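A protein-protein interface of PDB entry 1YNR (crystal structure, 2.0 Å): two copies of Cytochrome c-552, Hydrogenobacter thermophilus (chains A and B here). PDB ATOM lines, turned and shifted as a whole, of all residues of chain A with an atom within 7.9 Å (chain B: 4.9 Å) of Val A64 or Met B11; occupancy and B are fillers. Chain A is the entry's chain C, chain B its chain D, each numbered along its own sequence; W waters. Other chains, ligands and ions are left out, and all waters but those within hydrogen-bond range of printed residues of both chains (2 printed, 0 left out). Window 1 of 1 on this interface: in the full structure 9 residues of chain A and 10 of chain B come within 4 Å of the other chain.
The side-chain amino group of Lys A8 sits at hydrogen-bond distance from the backbone carbonyl oxygen of Asn A63 (2.8 Å).
The side-chain amino group (NZ) of Lys A47 lies within salt-bridge range of the side-chain carboxylate (OD2) of Asp A66 (3.3 Å).
The backbone carbonyl oxygen of Met B11 lies within hydrogen-bond range of the side-chain amino group of Lys B20.
The backbone NH (N) of Cys B10 sits at hydrogen-bond distance from the backbone carbonyl oxygen (O) of Ala B5, 3.0 Å away.
The backbone carbonyl oxygen of Asp B15 sits at hydrogen-bond distance from the backbone NH of Tyr B25.
OE1 of Glu A68 is in salt-bridge range of NZ of Lys A8.
The side-chain amide oxygen of Asn A63 lies within hydrogen-bond range of the backbone NH of Met B11.
The side-chain carboxylate (OE2) of Glu A68 lies within salt-bridge range of the side-chain amino group (NZ) of Lys B6 (2.8 Å).
The backbone carbonyl oxygen of Gln A62 sits close to the backbone carbonyl oxygen of Met B11 (3.3 Å).
The side-chain amino group (NZ) of Lys A47 is in salt-bridge range of the side-chain carboxylate (OD1) of Asp B15, at 3.4 Å.
O of Gln A62 lies within hydrogen-bond range of NZ of Lys B20 (2.9 Å).
ND2 of Asn A63 lies within hydrogen-bond range of O of Lys B6 (2.8 Å).
The backbone carbonyl oxygen (O) of Lys A47 is in hydrogen-bond range of the side-chain amino group (NZ) of Lys B20, at 3.0 Å.
The side-chain amide oxygen (OD1) of Asn A63 sits close to the backbone carbonyl oxygen (O) of Gly B9, 3.5 Å away.
N of Ala B12 sits at hydrogen-bond distance from OD1 of Asn A63, 3.3 Å away.
Among the printed residues, pairs that only touch across the chains: Lys A8 with Lys B6 (3.6 Å), Pro A61 with Ala B12 (3.1 Å), Gln A62 with Ala B12 (3.7 Å), Asn A63 with Cys B10 (3.7 Å), Val A64 with Met B11 (3.8 Å), Thr A65 with Glu B2 (3.9 Å) and Thr A65 with Lys B6 (3.6 Å).
Water W2 lies within hydrogen-bond range of the backbone carbonyl oxygen of Val A64, the side-chain amino group of Lys B20 and the side-chain carboxylate of Asp B15.
Water W1 lies within hydrogen-bond range of the backbone NH of Asp A66 (2.9 Å) and the side-chain carboxylate of Glu B2 (3.1 Å).
Positions printed for both chains: 5, 9 and 10.
Of the 16 pairs that touch across the chains among the printed residues, none has its exchanged pair printed and touching as well.
Hydrophobic or aromatic side chains of chain A within 4 Å of the printed part of chain B: Pro A61.
Hydrophobic or aromatic side chains of chain B within 4 Å of the printed part of chain A: Met B11.
Along chain B the printed residues that touch a printed residue of chain A span positions 2 to 20.
Among the printed residues, Asp or Glu carboxylates within 4 Å of a Lys or Arg side-chain nitrogen of the other chain: Lys A47 with Asp B15 and Glu A68 with Lys B6.
Leu A4 touches none of the printed residues of chain B.
Of the printed residues of chain B, Gln A62 touches Met B11 (3.3 Å), Ala B12 (3.7 Å) and Lys B20 (2.9 Å).
Of the printed residues of chain A, Cys B10 touches Asn A63.
Of chain A, only Pro A61, Gln A62 and Asn A63 come within 4 Å of Ala B12.
Of the printed residues of chain A, Asp B15 touches Lys A47.
The nearest residue of chain A that does not touch Met B11 is Thr A65 (4.9 Å).
The nearest printed residue of chain A that does not touch Lys B20 is Lys A48 (4.02 Å).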
ATOM      1  N   LEU A   4      18.651 -14.063  -4.059  1.00  0.00           N
ATOM      2  CA  LEU A   4      18.076 -13.857  -2.731  1.00  0.00           C
ATOM      3  C   LEU A   4      17.142 -12.649  -2.702  1.00  0.00           C
ATOM      4  O   LEU A   4      16.031 -12.724  -2.175  1.00  0.00           O
ATOM      5  CB  LEU A   4      19.187 -13.668  -1.680  1.00  0.00           C
ATOM      6  CG  LEU A   4      18.795 -13.434  -0.212  1.00  0.00           C
ATOM      7  CD1 LEU A   4      17.988 -14.642   0.302  1.00  0.00           C
ATOM      8  CD2 LEU A   4      20.062 -13.272   0.633  1.00  0.00           C
ATOM      9  N   ALA A   5      17.598 -11.523  -3.243  1.00  0.00           N
ATOM     10  CA  ALA A   5      16.753 -10.358  -3.352  1.00  0.00           C
ATOM     11  C   ALA A   5      15.416 -10.657  -4.054  1.00  0.00           C
ATOM     12  O   ALA A   5      14.344 -10.223  -3.583  1.00  0.00           O
ATOM     13  CB  ALA A   5      17.491  -9.239  -4.047  1.00  0.00           C
ATOM     14  N   LYS A   8      13.154 -12.969  -1.827  1.00  0.00           N
ATOM     15  CA  LYS A   8      12.530 -12.275  -0.696  1.00  0.00           C
ATOM     16  C   LYS A   8      11.439 -11.330  -1.107  1.00  0.00           C
ATOM     17  O   LYS A   8      10.663 -10.875  -0.249  1.00  0.00           O
ATOM     18  CB  LYS A   8      13.559 -11.482   0.134  1.00  0.00           C
ATOM     19  CG  LYS A   8      14.567 -12.331   0.877  1.00  0.00           C
ATOM     20  CD  LYS A   8      13.926 -13.260   1.924  1.00  0.00           C
ATOM     21  CE  LYS A   8      15.008 -13.920   2.809  1.00  0.00           C
ATOM     22  NZ  LYS A   8      14.453 -14.675   3.977  1.00  0.00           N
ATOM     23  N   GLY A   9      11.392 -10.992  -2.395  1.00  0.00           N
ATOM     24  CA  GLY A   9      10.394 -10.060  -2.907  1.00  0.00           C
ATOM     25  C   GLY A   9      10.833  -8.618  -3.089  1.00  0.00           C
ATOM     26  O   GLY A   9      10.008  -7.743  -3.382  1.00  0.00           O
ATOM     27  N   CYS A  10      12.122  -8.367  -2.898  1.00  0.00           N
ATOM     28  CA  CYS A  10      12.719  -7.023  -2.991  1.00  0.00           C
ATOM     29  C   CYS A  10      12.449  -6.360  -4.330  1.00  0.00           C
ATOM     30  O   CYS A  10      12.230  -5.163  -4.374  1.00  0.00           O
ATOM     31  CB  CYS A  10      14.245  -7.111  -2.810  1.00  0.00           C
ATOM     32  SG  CYS A  10      14.749  -7.942  -1.309  1.00  0.00           S
ATOM     33  N   ALA A  43      22.035  -2.984   6.172  1.00  0.00           N
ATOM     34  CA  ALA A  43      21.441  -4.178   6.781  1.00  0.00           C
ATOM     35  C   ALA A  43      20.284  -3.830   7.738  1.00  0.00           C
ATOM     36  O   ALA A  43      19.227  -4.455   7.700  1.00  0.00           O
ATOM     37  CB  ALA A  43      22.493  -5.014   7.496  1.00  0.00           C
ATOM     38  N   GLY A  44      20.508  -2.848   8.601  1.00  0.00           N
ATOM     39  CA  GLY A  44      19.470  -2.337   9.508  1.00  0.00           C
ATOM     40  C   GLY A  44      18.211  -1.892   8.766  1.00  0.00           C
ATOM     41  O   GLY A  44      17.093  -2.204   9.189  1.00  0.00           O
ATOM     42  N   LYS A  45      18.403  -1.165   7.664  1.00  0.00           N
ATOM     43  CA  LYS A  45      17.309  -0.616   6.870  1.00  0.00           C
ATOM     44  C   LYS A  45      16.558  -1.713   6.109  1.00  0.00           C
ATOM     45  O   LYS A  45      15.361  -1.603   5.896  1.00  0.00           O
ATOM     46  CB  LYS A  45      17.808   0.442   5.875  1.00  0.00           C
ATOM     47  CG  LYS A  45      18.568   1.652   6.485  1.00  0.00           C
ATOM     48  CD  LYS A  45      17.766   2.387   7.565  1.00  0.00           C
ATOM     49  CE  LYS A  45      16.464   2.957   7.015  1.00  0.00           C
ATOM     50  NZ  LYS A  45      16.672   4.064   6.020  1.00  0.00           N
ATOM     51  N   ILE A  46      17.283  -2.738   5.664  1.00  0.00           N
ATOM     52  CA  ILE A  46      16.676  -3.893   4.992  1.00  0.00           C
ATOM     53  C   ILE A  46      15.794  -4.694   5.976  1.00  0.00           C
ATOM     54  O   ILE A  46      14.699  -5.079   5.631  1.00  0.00           O
ATOM     55  CB  ILE A  46      17.793  -4.772   4.360  1.00  0.00           C
ATOM     56  CG1 ILE A  46      18.483  -3.934   3.252  1.00  0.00           C
ATOM     57  CG2 ILE A  46      17.241  -6.147   3.943  1.00  0.00           C
ATOM     58  CD1 ILE A  46      19.746  -4.560   2.649  1.00  0.00           C
ATOM     59  N   LYS A  47      16.257  -4.880   7.210  1.00  0.00           N
ATOM     60  CA  LYS A  47      15.501  -5.625   8.223  1.00  0.00           C
ATOM     61  C   LYS A  47      14.291  -4.834   8.677  1.00  0.00           C
ATOM     62  O   LYS A  47      13.187  -5.362   8.747  1.00  0.00           O
ATOM     63  CB  LYS A  47      16.368  -5.861   9.448  1.00  0.00           C
ATOM     64  CG  LYS A  47      17.480  -6.807   9.214  1.00  0.00           C
ATOM     65  CD  LYS A  47      18.583  -6.710  10.276  1.00  0.00           C
ATOM     66  CE  LYS A  47      18.050  -6.761  11.692  1.00  0.00           C
ATOM     67  NZ  LYS A  47      19.169  -6.898  12.694  1.00  0.00           N
ATOM     68  N   LYS A  48      14.516  -3.561   8.967  1.00  0.00           N
ATOM     69  CA  LYS A  48      13.545  -2.747   9.677  1.00  0.00           C
ATOM     70  C   LYS A  48      12.712  -1.846   8.792  1.00  0.00           C
ATOM     71  O   LYS A  48      11.662  -1.336   9.223  1.00  0.00           O
ATOM     72  CB  LYS A  48      14.276  -1.885  10.699  1.00  0.00           C
ATOM     73  CG  LYS A  48      15.042  -2.718  11.712  1.00  0.00           C
ATOM     74  CD  LYS A  48      15.703  -1.837  12.776  1.00  0.00           C
ATOM     75  CE  LYS A  48      14.713  -0.828  13.357  1.00  0.00           C
ATOM     76  NZ  LYS A  48      13.936  -1.392  14.517  1.00  0.00           N
ATOM     77  N   MET A  59       9.326   2.006   3.545  1.00  0.00           N
ATOM     78  CA  MET A  59       9.618   0.611   3.286  1.00  0.00           C
ATOM     79  C   MET A  59       9.185  -0.197   4.517  1.00  0.00           C
ATOM     80  O   MET A  59       9.509   0.189   5.656  1.00  0.00           O
ATOM     81  CB  MET A  59      11.123   0.402   3.081  1.00  0.00           C
ATOM     82  CG  MET A  59      11.500  -1.058   2.844  1.00  0.00           C
ATOM     83  SD  MET A  59      13.219  -1.289   2.406  1.00  0.00           S
ATOM     84  CE  MET A  59      13.398  -2.916   3.156  1.00  0.00           C
ATOM     85  N   PRO A  61       9.163  -3.504   7.122  1.00  0.00           N
ATOM     86  CA  PRO A  61      10.216  -4.407   7.595  1.00  0.00           C
ATOM     87  C   PRO A  61      10.154  -5.681   6.783  1.00  0.00           C
ATOM     88  O   PRO A  61       9.100  -5.991   6.187  1.00  0.00           O
ATOM     89  CB  PRO A  61       9.851  -4.668   9.071  1.00  0.00           C
ATOM     90  CG  PRO A  61       8.385  -4.442   9.149  1.00  0.00           C
ATOM     91  CD  PRO A  61       8.082  -3.334   8.120  1.00  0.00           C
ATOM     92  N   GLN A  62      11.275  -6.411   6.741  1.00  0.00           N
ATOM     93  CA  GLN A  62      11.433  -7.540   5.816  1.00  0.00           C
ATOM     94  C   GLN A  62      11.742  -8.829   6.526  1.00  0.00           C
ATOM     95  O   GLN A  62      12.363  -8.818   7.588  1.00  0.00           O
ATOM     96  CB  GLN A  62      12.540  -7.225   4.788  1.00  0.00           C
ATOM     97  CG  GLN A  62      12.231  -5.946   4.010  1.00  0.00           C
ATOM     98  CD  GLN A  62      11.018  -6.153   3.093  1.00  0.00           C
ATOM     99  OE1 GLN A  62      10.900  -7.200   2.449  1.00  0.00           O
ATOM    100  NE2 GLN A  62      10.114  -5.176   3.048  1.00  0.00           N
ATOM    101  N   ASN A  63      11.268  -9.935   5.936  1.00  0.00           N
ATOM    102  CA  ASN A  63      11.426 -11.278   6.497  1.00  0.00           C
ATOM    103  C   ASN A  63      12.826 -11.823   6.277  1.00  0.00           C
ATOM    104  O   ASN A  63      13.044 -12.775   5.495  1.00  0.00           O
ATOM    105  CB  ASN A  63      10.388 -12.213   5.875  1.00  0.00           C
ATOM    106  CG  ASN A  63      10.307 -13.546   6.554  1.00  0.00           C
ATOM    107  OD1 ASN A  63      10.350 -13.650   7.796  1.00  0.00           O
ATOM    108  ND2 ASN A  63      10.162 -14.601   5.742  1.00  0.00           N
ATOM    109  N   VAL A  64      13.794 -11.206   6.947  1.00  0.00           N
ATOM    110  CA  VAL A  64      15.190 -11.565   6.714  1.00  0.00           C
ATOM    111  C   VAL A  64      15.890 -11.766   8.045  1.00  0.00           C
ATOM    112  O   VAL A  64      15.553 -11.097   9.026  1.00  0.00           O
ATOM    113  CB  VAL A  64      15.961 -10.520   5.819  1.00  0.00           C
ATOM    114  CG1 VAL A  64      15.341 -10.392   4.392  1.00  0.00           C
ATOM    115  CG2 VAL A  64      16.073  -9.150   6.521  1.00  0.00           C
ATOM    116  N   THR A  65      16.817 -12.732   8.086  1.00  0.00           N
ATOM    117  CA  THR A  65      17.713 -12.885   9.218  1.00  0.00           C
ATOM    118  C   THR A  65      18.768 -11.787   9.116  1.00  0.00           C
ATOM    119  O   THR A  65      18.855 -11.097   8.095  1.00  0.00           O
ATOM    120  CB  THR A  65      18.420 -14.245   9.172  1.00  0.00           C
ATOM    121  OG1 THR A  65      19.223 -14.307   7.992  1.00  0.00           O
ATOM    122  CG2 THR A  65      17.399 -15.415   9.162  1.00  0.00           C
ATOM    123  N   ASP A  66      19.591 -11.639  10.144  1.00  0.00           N
ATOM    124  CA  ASP A  66      20.613 -10.607  10.127  1.00  0.00           C
ATOM    125  C   ASP A  66      21.659 -10.948   9.056  1.00  0.00           C
ATOM    126  O   ASP A  66      22.168 -10.059   8.380  1.00  0.00           O
ATOM    127  CB  ASP A  66      21.247 -10.442  11.525  1.00  0.00           C
ATOM    128  CG  ASP A  66      22.271  -9.320  11.571  1.00  0.00           C
ATOM    129  OD1 ASP A  66      23.464  -9.643  11.703  1.00  0.00           O
ATOM    130  OD2 ASP A  66      21.913  -8.124  11.444  1.00  0.00           O
ATOM    131  N   ALA A  67      21.950 -12.243   8.906  1.00  0.00           N
ATOM    132  CA  ALA A  67      22.897 -12.726   7.897  1.00  0.00           C
ATOM    133  C   ALA A  67      22.388 -12.406   6.494  1.00  0.00           C
ATOM    134  O   ALA A  67      23.136 -11.903   5.662  1.00  0.00           O
ATOM    135  CB  ALA A  67      23.162 -14.224   8.061  1.00  0.00           C
ATOM    136  N   GLU A  68      21.102 -12.667   6.242  1.00  0.00           N
ATOM    137  CA  GLU A  68      20.501 -12.314   4.947  1.00  0.00           C
ATOM    138  C   GLU A  68      20.531 -10.822   4.671  1.00  0.00           C
ATOM    139  O   GLU A  68      20.784 -10.424   3.547  1.00  0.00           O
ATOM    140  CB  GLU A  68      19.081 -12.850   4.832  1.00  0.00           C
ATOM    141  CG  GLU A  68      19.004 -14.349   4.509  1.00  0.00           C
ATOM    142  CD  GLU A  68      17.619 -14.908   4.734  1.00  0.00           C
ATOM    143  OE1 GLU A  68      16.807 -14.257   5.447  1.00  0.00           O
ATOM    144  OE2 GLU A  68      17.338 -16.022   4.239  1.00  0.00           O
ATOM    145  N   ALA A  69      20.272  -9.997   5.690  1.00  0.00           N
ATOM    146  CA  ALA A  69      20.292  -8.537   5.541  1.00  0.00           C
ATOM    147  C   ALA A  69      21.681  -8.051   5.138  1.00  0.00           C
ATOM    148  O   ALA A  69      21.824  -7.153   4.302  1.00  0.00           O
ATOM    149  CB  ALA A  69      19.869  -7.859   6.857  1.00  0.00           C
ATOM    150  N   LYS A  70      22.699  -8.620   5.770  1.00  0.00           N
ATOM    151  CA  LYS A  70      24.064  -8.264   5.452  1.00  0.00           C
ATOM    152  C   LYS A  70      24.453  -8.719   4.035  1.00  0.00           C
ATOM    153  O   LYS A  70      25.114  -7.962   3.315  1.00  0.00           O
ATOM    154  CB  LYS A  70      25.041  -8.770   6.520  1.00  0.00           C
ATOM    155  CG  LYS A  70      24.726  -8.216   7.913  1.00  0.00           C
ATOM    156  CD  LYS A  70      25.906  -7.550   8.584  1.00  0.00           C
ATOM    157  CE  LYS A  70      25.519  -6.930   9.942  1.00  0.00           C
ATOM    158  NZ  LYS A  70      25.607  -7.946  11.048  1.00  0.00           N
ATOM    159  N   LEU A  72      22.389  -9.050   1.492  1.00  0.00           N
ATOM    160  CA  LEU A  72      21.665  -8.173   0.604  1.00  0.00           C
ATOM    161  C   LEU A  72      22.280  -6.759   0.536  1.00  0.00           C
ATOM    162  O   LEU A  72      22.354  -6.171  -0.530  1.00  0.00           O
ATOM    163  CB  LEU A  72      20.183  -8.133   1.021  1.00  0.00           C
ATOM    164  CG  LEU A  72      19.453  -9.443   0.650  1.00  0.00           C
ATOM    165  CD1 LEU A  72      18.158  -9.553   1.453  1.00  0.00           C
ATOM    166  CD2 LEU A  72      19.145  -9.473  -0.848  1.00  0.00           C
ATOM    167  N   GLU B   2      14.878 -21.265  13.774  1.00  0.00           N
ATOM    168  CA  GLU B   2      14.993 -19.967  13.103  1.00  0.00           C
ATOM    169  C   GLU B   2      14.603 -20.122  11.641  1.00  0.00           C
ATOM    170  O   GLU B   2      14.026 -19.206  11.048  1.00  0.00           O
ATOM    171  CB  GLU B   2      16.386 -19.330  13.232  1.00  0.00           C
ATOM    172  CG  GLU B   2      16.453 -17.963  12.500  1.00  0.00           C
ATOM    173  CD  GLU B   2      17.689 -17.120  12.792  1.00  0.00           C
ATOM    174  OE1 GLU B   2      18.807 -17.655  12.715  1.00  0.00           O
ATOM    175  OE2 GLU B   2      17.533 -15.899  13.076  1.00  0.00           O
ATOM    176  N   ALA B   5      10.796 -20.258  11.551  1.00  0.00           N
ATOM    177  CA  ALA B   5      10.297 -18.876  11.755  1.00  0.00           C
ATOM    178  C   ALA B   5      10.348 -18.082  10.443  1.00  0.00           C
ATOM    179  O   ALA B   5       9.379 -17.416  10.079  1.00  0.00           O
ATOM    180  CB  ALA B   5      11.058 -18.160  12.865  1.00  0.00           C
ATOM    181  N   LYS B   6      11.474 -18.171   9.728  1.00  0.00           N
ATOM    182  CA  LYS B   6      11.646 -17.423   8.482  1.00  0.00           C
ATOM    183  C   LYS B   6      10.656 -17.969   7.442  1.00  0.00           C
ATOM    184  O   LYS B   6       9.970 -17.232   6.717  1.00  0.00           O
ATOM    185  CB  LYS B   6      13.079 -17.600   7.986  1.00  0.00           C
ATOM    186  CG  LYS B   6      13.609 -16.490   7.139  1.00  0.00           C
ATOM    187  CD  LYS B   6      15.067 -16.803   6.752  1.00  0.00           C
ATOM    188  CE  LYS B   6      15.236 -18.102   6.018  1.00  0.00           C
ATOM    189  NZ  LYS B   6      16.663 -18.327   5.698  1.00  0.00           N
ATOM    190  N   GLY B   9       7.294 -16.425   7.787  1.00  0.00           N
ATOM    191  CA  GLY B   9       7.146 -14.988   7.642  1.00  0.00           C
ATOM    192  C   GLY B   9       7.318 -14.211   8.927  1.00  0.00           C
ATOM    193  O   GLY B   9       7.131 -13.012   8.933  1.00  0.00           O
ATOM    194  N   CYS B  10       7.709 -14.890  10.010  1.00  0.00           N
ATOM    195  CA  CYS B  10       7.767 -14.282  11.351  1.00  0.00           C
ATOM    196  C   CYS B  10       8.790 -13.159  11.465  1.00  0.00           C
ATOM    197  O   CYS B  10       8.568 -12.206  12.214  1.00  0.00           O
ATOM    198  CB  CYS B  10       8.135 -15.343  12.434  1.00  0.00           C
ATOM    199  SG  CYS B  10       7.099 -16.797  12.473  1.00  0.00           S
ATOM    200  N   MET B  11       9.907 -13.306  10.756  1.00  0.00           N
ATOM    201  CA  MET B  11      10.993 -12.337  10.809  1.00  0.00           C
ATOM    202  C   MET B  11      10.596 -10.992  10.240  1.00  0.00           C
ATOM    203  O   MET B  11      11.295 -10.021  10.512  1.00  0.00           O
ATOM    204  CB  MET B  11      12.272 -12.796  10.084  1.00  0.00           C
ATOM    205  CG  MET B  11      12.595 -14.283  10.138  1.00  0.00           C
ATOM    206  SD  MET B  11      12.634 -14.889  11.799  1.00  0.00           S
ATOM    207  CE  MET B  11      14.026 -13.899  12.364  1.00  0.00           C
ATOM    208  N   ALA B  12       9.520 -10.910   9.440  1.00  0.00           N
ATOM    209  CA  ALA B  12       9.066  -9.586   8.968  1.00  0.00           C
ATOM    210  C   ALA B  12       8.743  -8.683  10.134  1.00  0.00           C
ATOM    211  O   ALA B  12       9.004  -7.483  10.063  1.00  0.00           O
ATOM    212  CB  ALA B  12       7.850  -9.682   8.066  1.00  0.00           C
ATOM    213  N   CYS B  13       8.194  -9.243  11.214  1.00  0.00           N
ATOM    214  CA  CYS B  13       7.860  -8.420  12.400  1.00  0.00           C
ATOM    215  C   CYS B  13       8.732  -8.610  13.645  1.00  0.00           C
ATOM    216  O   CYS B  13       8.665  -7.813  14.594  1.00  0.00           O
ATOM    217  CB  CYS B  13       6.431  -8.705  12.814  1.00  0.00           C
ATOM    218  SG  CYS B  13       5.195  -8.126  11.589  1.00  0.00           S
ATOM    219  N   HIS B  14       9.525  -9.671  13.643  1.00  0.00           N
ATOM    220  CA  HIS B  14      10.373  -9.996  14.781  1.00  0.00           C
ATOM    221  C   HIS B  14      11.823 -10.198  14.383  1.00  0.00           C
ATOM    222  O   HIS B  14      12.127 -10.977  13.462  1.00  0.00           O
ATOM    223  CB  HIS B  14       9.910 -11.307  15.430  1.00  0.00           C
ATOM    224  CG  HIS B  14       8.543 -11.265  16.038  1.00  0.00           C
ATOM    225  ND1 HIS B  14       8.305 -10.759  17.297  1.00  0.00           N
ATOM    226  CD2 HIS B  14       7.346 -11.698  15.569  1.00  0.00           C
ATOM    227  CE1 HIS B  14       7.015 -10.898  17.581  1.00  0.00           C
ATOM    228  NE2 HIS B  14       6.407 -11.444  16.538  1.00  0.00           N
ATOM    229  N   ASP B  15      12.717  -9.524  15.089  1.00  0.00           N
ATOM    230  CA  ASP B  15      14.135  -9.790  14.966  1.00  0.00           C
ATOM    231  C   ASP B  15      14.560 -10.560  16.224  1.00  0.00           C
ATOM    232  O   ASP B  15      13.837 -10.545  17.217  1.00  0.00           O
ATOM    233  CB  ASP B  15      14.895  -8.467  14.843  1.00  0.00           C
ATOM    234  CG  ASP B  15      16.343  -8.668  14.457  1.00  0.00           C
ATOM    235  OD1 ASP B  15      16.623  -9.079  13.291  1.00  0.00           O
ATOM    236  OD2 ASP B  15      17.203  -8.409  15.324  1.00  0.00           O
ATOM    237  N   LYS B  20      11.300  -4.440  15.863  1.00  0.00           N
ATOM    238  CA  LYS B  20      10.768  -4.128  14.551  1.00  0.00           C
ATOM    239  C   LYS B  20       9.302  -3.801  14.754  1.00  0.00           C
ATOM    240  O   LYS B  20       8.953  -2.619  14.990  1.00  0.00           O
ATOM    241  CB  LYS B  20      10.975  -5.288  13.546  1.00  0.00           C
ATOM    242  CG  LYS B  20      12.442  -5.757  13.455  1.00  0.00           C
ATOM    243  CD  LYS B  20      12.882  -6.098  12.028  1.00  0.00           C
ATOM    244  CE  LYS B  20      12.145  -7.320  11.506  1.00  0.00           C
ATOM    245  NZ  LYS B  20      12.904  -7.899  10.321  1.00  0.00           N
ATOM    246  N   TYR B  25      12.793 -11.643  19.686  1.00  0.00           N
ATOM    247  CA  TYR B  25      12.716 -12.982  20.272  1.00  0.00           C
ATOM    248  C   TYR B  25      13.492 -13.133  21.601  1.00  0.00           C
ATOM    249  O   TYR B  25      13.028 -13.830  22.492  1.00  0.00           O
ATOM    250  CB  TYR B  25      13.148 -14.049  19.268  1.00  0.00           C
ATOM    251  CG  TYR B  25      12.487 -14.152  17.914  1.00  0.00           C
ATOM    252  CD1 TYR B  25      13.242 -14.026  16.743  1.00  0.00           C
ATOM    253  CD2 TYR B  25      11.143 -14.485  17.802  1.00  0.00           C
ATOM    254  CE1 TYR B  25      12.650 -14.162  15.489  1.00  0.00           C
ATOM    255  CE2 TYR B  25      10.546 -14.609  16.580  1.00  0.00           C
ATOM    256  CZ  TYR B  25      11.293 -14.439  15.423  1.00  0.00           C
ATOM    257  OH  TYR B  25      10.674 -14.587  14.217  1.00  0.00           O
HETATM  258  O   HOH W   1      18.925 -13.166  12.553  1.00  0.00           O
HETATM  259  O   HOH W   2      15.215  -9.240  10.756  1.00  0.00           O
